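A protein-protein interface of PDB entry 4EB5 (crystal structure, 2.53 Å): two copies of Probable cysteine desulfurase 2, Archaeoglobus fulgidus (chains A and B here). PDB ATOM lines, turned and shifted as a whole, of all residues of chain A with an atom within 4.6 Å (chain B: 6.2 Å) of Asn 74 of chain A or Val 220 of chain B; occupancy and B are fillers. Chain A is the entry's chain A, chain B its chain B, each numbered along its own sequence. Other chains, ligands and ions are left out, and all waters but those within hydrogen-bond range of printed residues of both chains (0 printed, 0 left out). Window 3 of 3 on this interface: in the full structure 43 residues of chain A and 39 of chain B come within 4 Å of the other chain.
Asn 74 of chain A touches just these residues of chain B: Val 220, Ile 221 and Leu 222. Of chain A, only Asn 74 and Val 220 come within 4 Å of Val 220 of chain B. Printed residues of chain A within 4 Å of Asn 74 of chain B: Val 220 (3.999 Å). Printed residues of chain A within 4 Å of Gly 223 of chain B: Ser 100 (3.9 Å). Of the printed residues of chain B, Glu 71 of chain A touches Ile 221. Of the printed residues of chain B, Val 220 of chain A touches Asn 74 and Val 220. Pro 219 of chain B touches none of the printed residues of chain A.
ND2 of Asn 74 of chain A is in hydrogen-bond range of O of Leu 222 of chain B (2.6 Å).
ND2 of Asn 74 of chain A sits at hydrogen-bond distance from O of Thr 70 of chain A, 2.9 Å away. ND2 of Asn 73 of chain A lies within hydrogen-bond range of OG of Ser 100 of chain A, 3.1 Å away.
Asn 74 of chain A touches Val 220 of chain B, and with the chains exchanged Val 220 of chain A touches Asn 74 of chain B. Val 220 of chain B touches its own counterpart, Val 220 of chain A. Positions printed for both chains: 74, 75, 78, 79 and 220.
Among the printed residues, pairs that only touch across the chains: Thr 70 of chain A with Ile 221 of chain B (3.9 Å), Thr 70 of chain A with Leu 222 of chain B (3.8 Å), Glu 71 of chain A with Ile 221 of chain B (3.8 Å), Asn 74 of chain A with Val 220 of chain B (3.9 Å), Asn 74 of chain A with Ile 221 of chain B (3.7 Å), Ser 100 of chain A with Leu 222 of chain B (3.9 Å), Ser 100 of chain A with Gly 223 of chain B (3.9 Å), Pro 104 of chain A with Leu 222 of chain B (3.99 Å), Val 220 of chain A with Asn 74 of chain B (3.999 Å) and Val 220 of chain A with Val 220 of chain B (3.8 Å).
Of the 11 printed residues of chain B, 5 touch a printed residue of chain A. Printed residues of chain B that touch a printed residue of chain A: Asn 74, Val 220, Ile 221, Leu 222 and Gly 223. Along chain B the printed residues that touch a printed residue of chain A span positions 74 to 223. Hydrophobic or aromatic side chains of chain A that line the printed part of chain B: Pro 104 and Val 220. Among the printed residues, 11 pairs touch across the chains. Among the printed residues, no Asp or Glu carboxylate lies within 4 Å of a Lys or Arg side-chain nitrogen of the other chain.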
ATOM      1  N   THR A  70      11.159 -18.719  11.561  1.00  0.00           N
ATOM      2  CA  THR A  70      10.866 -19.215  12.875  1.00  0.00           C
ATOM      3  C   THR A  70       9.723 -20.236  12.839  1.00  0.00           C
ATOM      4  O   THR A  70       9.884 -21.363  13.318  1.00  0.00           O
ATOM      5  CB  THR A  70      10.683 -18.057  13.863  1.00  0.00           C
ATOM      6  OG1 THR A  70      11.961 -17.430  14.045  1.00  0.00           O
ATOM      7  CG2 THR A  70      10.204 -18.552  15.192  1.00  0.00           C
ATOM      8  N   GLU A  71       8.610 -19.863  12.223  1.00  0.00           N
ATOM      9  CA  GLU A  71       7.472 -20.762  12.066  1.00  0.00           C
ATOM     10  C   GLU A  71       7.774 -22.029  11.227  1.00  0.00           C
ATOM     11  O   GLU A  71       7.335 -23.131  11.580  1.00  0.00           O
ATOM     12  CB  GLU A  71       6.287 -20.004  11.456  1.00  0.00           C
ATOM     13  CG  GLU A  71       5.001 -20.797  11.449  1.00  0.00           C
ATOM     14  CD  GLU A  71       3.950 -20.151  10.639  1.00  0.00           C
ATOM     15  OE1 GLU A  71       3.980 -18.912  10.486  1.00  0.00           O
ATOM     16  OE2 GLU A  71       3.082 -20.891  10.134  1.00  0.00           O
ATOM     17  N   ALA A  72       8.510 -21.854  10.119  1.00  0.00           N
ATOM     18  CA  ALA A  72       8.940 -22.957   9.264  1.00  0.00           C
ATOM     19  C   ALA A  72       9.822 -23.957  10.025  1.00  0.00           C
ATOM     20  O   ALA A  72       9.681 -25.177   9.853  1.00  0.00           O
ATOM     21  CB  ALA A  72       9.634 -22.441   8.030  1.00  0.00           C
ATOM     22  N   ASN A  73      10.719 -23.441  10.859  1.00  0.00           N
ATOM     23  CA  ASN A  73      11.526 -24.280  11.749  1.00  0.00           C
ATOM     24  C   ASN A  73      10.637 -25.019  12.764  1.00  0.00           C
ATOM     25  O   ASN A  73      10.862 -26.190  13.049  1.00  0.00           O
ATOM     26  CB  ASN A  73      12.609 -23.454  12.458  1.00  0.00           C
ATOM     27  CG  ASN A  73      13.864 -23.301  11.623  1.00  0.00           C
ATOM     28  OD1 ASN A  73      14.039 -23.995  10.613  1.00  0.00           O
ATOM     29  ND2 ASN A  73      14.755 -22.396  12.033  1.00  0.00           N
ATOM     30  N   ASN A  74       9.627 -24.310  13.279  1.00  0.00           N
ATOM     31  CA  ASN A  74       8.706 -24.878  14.218  1.00  0.00           C
ATOM     32  C   ASN A  74       7.888 -26.004  13.595  1.00  0.00           C
ATOM     33  O   ASN A  74       7.621 -27.016  14.252  1.00  0.00           O
ATOM     34  CB  ASN A  74       7.742 -23.813  14.738  1.00  0.00           C
ATOM     35  CG  ASN A  74       8.186 -23.198  16.028  1.00  0.00           C
ATOM     36  OD1 ASN A  74       7.570 -23.397  17.067  1.00  0.00           O
ATOM     37  ND2 ASN A  74       9.254 -22.432  15.972  1.00  0.00           N
ATOM     38  N   LEU A  75       7.481 -25.799  12.334  1.00  0.00           N
ATOM     39  CA  LEU A  75       6.638 -26.731  11.616  1.00  0.00           C
ATOM     40  C   LEU A  75       7.450 -27.939  11.220  1.00  0.00           C
ATOM     41  O   LEU A  75       6.972 -29.059  11.294  1.00  0.00           O
ATOM     42  CB  LEU A  75       6.047 -26.066  10.377  1.00  0.00           C
ATOM     43  CG  LEU A  75       5.380 -26.928   9.295  1.00  0.00           C
ATOM     44  CD1 LEU A  75       4.200 -27.729   9.858  1.00  0.00           C
ATOM     45  CD2 LEU A  75       4.919 -26.059   8.153  1.00  0.00           C
ATOM     46  N   ALA A  76       8.689 -27.720  10.821  1.00  0.00           N
ATOM     47  CA  ALA A  76       9.524 -28.829  10.394  1.00  0.00           C
ATOM     48  C   ALA A  76       9.869 -29.775  11.525  1.00  0.00           C
ATOM     49  O   ALA A  76       9.985 -30.973  11.298  1.00  0.00           O
ATOM     50  CB  ALA A  76      10.803 -28.321   9.749  1.00  0.00           C
ATOM     51  N   ILE A  77      10.086 -29.223  12.719  1.00  0.00           N
ATOM     52  CA  ILE A  77      10.513 -30.010  13.886  1.00  0.00           C
ATOM     53  C   ILE A  77       9.311 -30.664  14.559  1.00  0.00           C
ATOM     54  O   ILE A  77       9.251 -31.900  14.637  1.00  0.00           O
ATOM     55  CB  ILE A  77      11.334 -29.166  14.897  1.00  0.00           C
ATOM     56  CG1 ILE A  77      12.682 -28.773  14.281  1.00  0.00           C
ATOM     57  CG2 ILE A  77      11.557 -29.928  16.219  1.00  0.00           C
ATOM     58  CD1 ILE A  77      13.574 -30.007  14.021  1.00  0.00           C
ATOM     59  N   ILE A  78       8.346 -29.844  15.007  1.00  0.00           N
ATOM     60  CA  ILE A  78       7.137 -30.343  15.636  1.00  0.00           C
ATOM     61  C   ILE A  78       6.282 -31.098  14.622  1.00  0.00           C
ATOM     62  O   ILE A  78       5.890 -32.228  14.868  1.00  0.00           O
ATOM     63  CB  ILE A  78       6.354 -29.223  16.404  1.00  0.00           C
ATOM     64  CG1 ILE A  78       7.198 -28.767  17.596  1.00  0.00           C
ATOM     65  CG2 ILE A  78       4.938 -29.746  16.879  1.00  0.00           C
ATOM     66  CD1 ILE A  78       6.758 -27.501  18.266  1.00  0.00           C
ATOM     67  N   GLY A  79       6.045 -30.480  13.467  1.00  0.00           N
ATOM     68  CA  GLY A  79       5.188 -31.050  12.431  1.00  0.00           C
ATOM     69  C   GLY A  79       5.636 -32.378  11.888  1.00  0.00           C
ATOM     70  O   GLY A  79       4.817 -33.254  11.641  1.00  0.00           O
ATOM     71  N   SER A 100      14.948 -21.170  17.234  1.00  0.00           N
ATOM     72  CA  SER A 100      13.679 -21.624  16.598  1.00  0.00           C
ATOM     73  C   SER A 100      13.684 -23.088  16.144  1.00  0.00           C
ATOM     74  O   SER A 100      12.688 -23.615  15.643  1.00  0.00           O
ATOM     75  CB  SER A 100      13.303 -20.705  15.437  1.00  0.00           C
ATOM     76  OG  SER A 100      14.385 -20.584  14.536  1.00  0.00           O
ATOM     77  N   PRO A 104      11.568 -25.771  19.889  1.00  0.00           N
ATOM     78  CA  PRO A 104      10.674 -26.853  19.483  1.00  0.00           C
ATOM     79  C   PRO A 104      11.229 -28.218  19.869  1.00  0.00           C
ATOM     80  O   PRO A 104      10.478 -29.106  20.333  1.00  0.00           O
ATOM     81  CB  PRO A 104      10.621 -26.694  17.958  1.00  0.00           C
ATOM     82  CG  PRO A 104      10.855 -25.223  17.742  1.00  0.00           C
ATOM     83  CD  PRO A 104      11.824 -24.823  18.780  1.00  0.00           C
ATOM     84  N   VAL A 220       0.946 -27.093  12.322  1.00  0.00           N
ATOM     85  CA  VAL A 220       0.955 -26.406  13.608  1.00  0.00           C
ATOM     86  C   VAL A 220      -0.052 -25.279  13.669  1.00  0.00           C
ATOM     87  O   VAL A 220      -0.646 -25.091  14.700  1.00  0.00           O
ATOM     88  CB  VAL A 220       2.323 -25.845  13.972  1.00  0.00           C
ATOM     89  CG1 VAL A 220       2.193 -24.994  15.239  1.00  0.00           C
ATOM     90  CG2 VAL A 220       3.283 -26.971  14.221  1.00  0.00           C
ATOM     91  N   ASN B  74      -5.689 -19.518  17.336  1.00  0.00           N
ATOM     92  CA  ASN B  74      -4.943 -20.697  17.718  1.00  0.00           C
ATOM     93  C   ASN B  74      -4.240 -20.503  19.079  1.00  0.00           C
ATOM     94  O   ASN B  74      -4.191 -21.411  19.910  1.00  0.00           O
ATOM     95  CB  ASN B  74      -3.953 -21.073  16.594  1.00  0.00           C
ATOM     96  CG  ASN B  74      -4.572 -22.005  15.531  1.00  0.00           C
ATOM     97  OD1 ASN B  74      -4.055 -23.078  15.261  1.00  0.00           O
ATOM     98  ND2 ASN B  74      -5.686 -21.595  14.946  1.00  0.00           N
ATOM     99  N   LEU B  75      -3.755 -19.293  19.330  1.00  0.00           N
ATOM    100  CA  LEU B  75      -3.045 -19.003  20.560  1.00  0.00           C
ATOM    101  C   LEU B  75      -4.004 -18.862  21.781  1.00  0.00           C
ATOM    102  O   LEU B  75      -3.683 -19.266  22.893  1.00  0.00           O
ATOM    103  CB  LEU B  75      -2.160 -17.781  20.356  1.00  0.00           C
ATOM    104  CG  LEU B  75      -1.416 -17.219  21.572  1.00  0.00           C
ATOM    105  CD1 LEU B  75      -0.407 -18.209  22.195  1.00  0.00           C
ATOM    106  CD2 LEU B  75      -0.754 -15.939  21.182  1.00  0.00           C
ATOM    107  N   ILE B  78      -5.523 -22.820  22.336  1.00  0.00           N
ATOM    108  CA  ILE B  78      -4.538 -23.815  22.712  1.00  0.00           C
ATOM    109  C   ILE B  78      -3.563 -23.246  23.740  1.00  0.00           C
ATOM    110  O   ILE B  78      -3.248 -23.887  24.726  1.00  0.00           O
ATOM    111  CB  ILE B  78      -3.759 -24.213  21.482  1.00  0.00           C
ATOM    112  CG1 ILE B  78      -4.633 -24.996  20.517  1.00  0.00           C
ATOM    113  CG2 ILE B  78      -2.484 -24.928  21.855  1.00  0.00           C
ATOM    114  CD1 ILE B  78      -3.931 -25.200  19.178  1.00  0.00           C
ATOM    115  N   GLY B  79      -3.081 -22.034  23.505  1.00  0.00           N
ATOM    116  CA  GLY B  79      -2.226 -21.382  24.471  1.00  0.00           C
ATOM    117  C   GLY B  79      -2.897 -21.285  25.824  1.00  0.00           C
ATOM    118  O   GLY B  79      -2.260 -21.488  26.852  1.00  0.00           O
ATOM    119  N   GLN B 218       0.477 -20.236  27.312  1.00  0.00           N
ATOM    120  CA  GLN B 218       1.701 -20.854  26.829  1.00  0.00           C
ATOM    121  C   GLN B 218       1.862 -20.563  25.299  1.00  0.00           C
ATOM    122  O   GLN B 218       0.888 -20.590  24.547  1.00  0.00           O
ATOM    123  CB  GLN B 218       1.604 -22.349  27.115  1.00  0.00           C
ATOM    124  CG  GLN B 218       2.166 -23.249  26.031  1.00  0.00           C
ATOM    125  CD  GLN B 218       1.759 -24.687  26.223  1.00  0.00           C
ATOM    126  OE1 GLN B 218       1.720 -25.177  27.354  1.00  0.00           O
ATOM    127  NE2 GLN B 218       1.455 -25.374  25.125  1.00  0.00           N
ATOM    128  N   PRO B 219       3.092 -20.309  24.825  1.00  0.00           N
ATOM    129  CA  PRO B 219       3.267 -19.988  23.386  1.00  0.00           C
ATOM    130  C   PRO B 219       3.034 -21.151  22.418  1.00  0.00           C
ATOM    131  O   PRO B 219       3.280 -22.284  22.745  1.00  0.00           O
ATOM    132  CB  PRO B 219       4.724 -19.554  23.310  1.00  0.00           C
ATOM    133  CG  PRO B 219       5.388 -20.289  24.445  1.00  0.00           C
ATOM    134  CD  PRO B 219       4.377 -20.373  25.543  1.00  0.00           C
ATOM    135  N   VAL B 220       2.571 -20.865  21.218  1.00  0.00           N
ATOM    136  CA  VAL B 220       2.489 -21.903  20.207  1.00  0.00           C
ATOM    137  C   VAL B 220       3.703 -21.895  19.290  1.00  0.00           C
ATOM    138  O   VAL B 220       4.155 -22.976  18.878  1.00  0.00           O
ATOM    139  CB  VAL B 220       1.182 -21.861  19.380  1.00  0.00           C
ATOM    140  CG1 VAL B 220       1.256 -22.921  18.287  1.00  0.00           C
ATOM    141  CG2 VAL B 220      -0.043 -22.146  20.299  1.00  0.00           C
ATOM    142  N   ILE B 221       4.242 -20.697  18.990  1.00  0.00           N
ATOM    143  CA  ILE B 221       5.418 -20.564  18.138  1.00  0.00           C
ATOM    144  C   ILE B 221       6.604 -20.346  19.026  1.00  0.00           C
ATOM    145  O   ILE B 221       6.674 -19.338  19.722  1.00  0.00           O
ATOM    146  CB  ILE B 221       5.270 -19.397  17.128  1.00  0.00           C
ATOM    147  CG1 ILE B 221       3.967 -19.525  16.302  1.00  0.00           C
ATOM    148  CG2 ILE B 221       6.487 -19.309  16.196  1.00  0.00           C
ATOM    149  CD1 ILE B 221       4.050 -20.569  15.151  1.00  0.00           C
ATOM    150  N   LEU B 222       7.551 -21.277  18.997  1.00  0.00           N
ATOM    151  CA  LEU B 222       8.663 -21.313  19.945  1.00  0.00           C
ATOM    152  C   LEU B 222       9.913 -20.820  19.256  1.00  0.00           C
ATOM    153  O   LEU B 222      10.080 -21.029  18.043  1.00  0.00           O
ATOM    154  CB  LEU B 222       8.880 -22.729  20.463  1.00  0.00           C
ATOM    155  CG  LEU B 222       7.643 -23.478  20.990  1.00  0.00           C
ATOM    156  CD1 LEU B 222       8.059 -24.678  21.758  1.00  0.00           C
ATOM    157  CD2 LEU B 222       6.791 -22.608  21.905  1.00  0.00           C
ATOM    158  N   GLY B 223      10.773 -20.135  20.020  1.00  0.00           N
ATOM    159  CA  GLY B 223      12.014 -19.604  19.491  1.00  0.00           C
ATOM    160  C   GLY B 223      12.826 -18.682  20.379  1.00  0.00           C
ATOM    161  O   GLY B 223      13.144 -19.014  21.533  1.00  0.00           O
ATOM    162  N   LEU B 230       5.798 -14.999  24.262  1.00  0.00           N
ATOM    163  CA  LEU B 230       4.523 -15.446  23.801  1.00  0.00           C
ATOM    164  C   LEU B 230       4.476 -15.759  22.302  1.00  0.00           C
ATOM    165  O   LEU B 230       3.639 -16.547  21.872  1.00  0.00           O
ATOM    166  CB  LEU B 230       3.504 -14.386  24.182  1.00  0.00           C
ATOM    167  CG  LEU B 230       3.182 -14.428  25.689  1.00  0.00           C
ATOM    168  CD1 LEU B 230       2.789 -13.054  26.213  1.00  0.00           C
ATOM    169  CD2 LEU B 230       2.117 -15.534  26.054  1.00  0.00           C
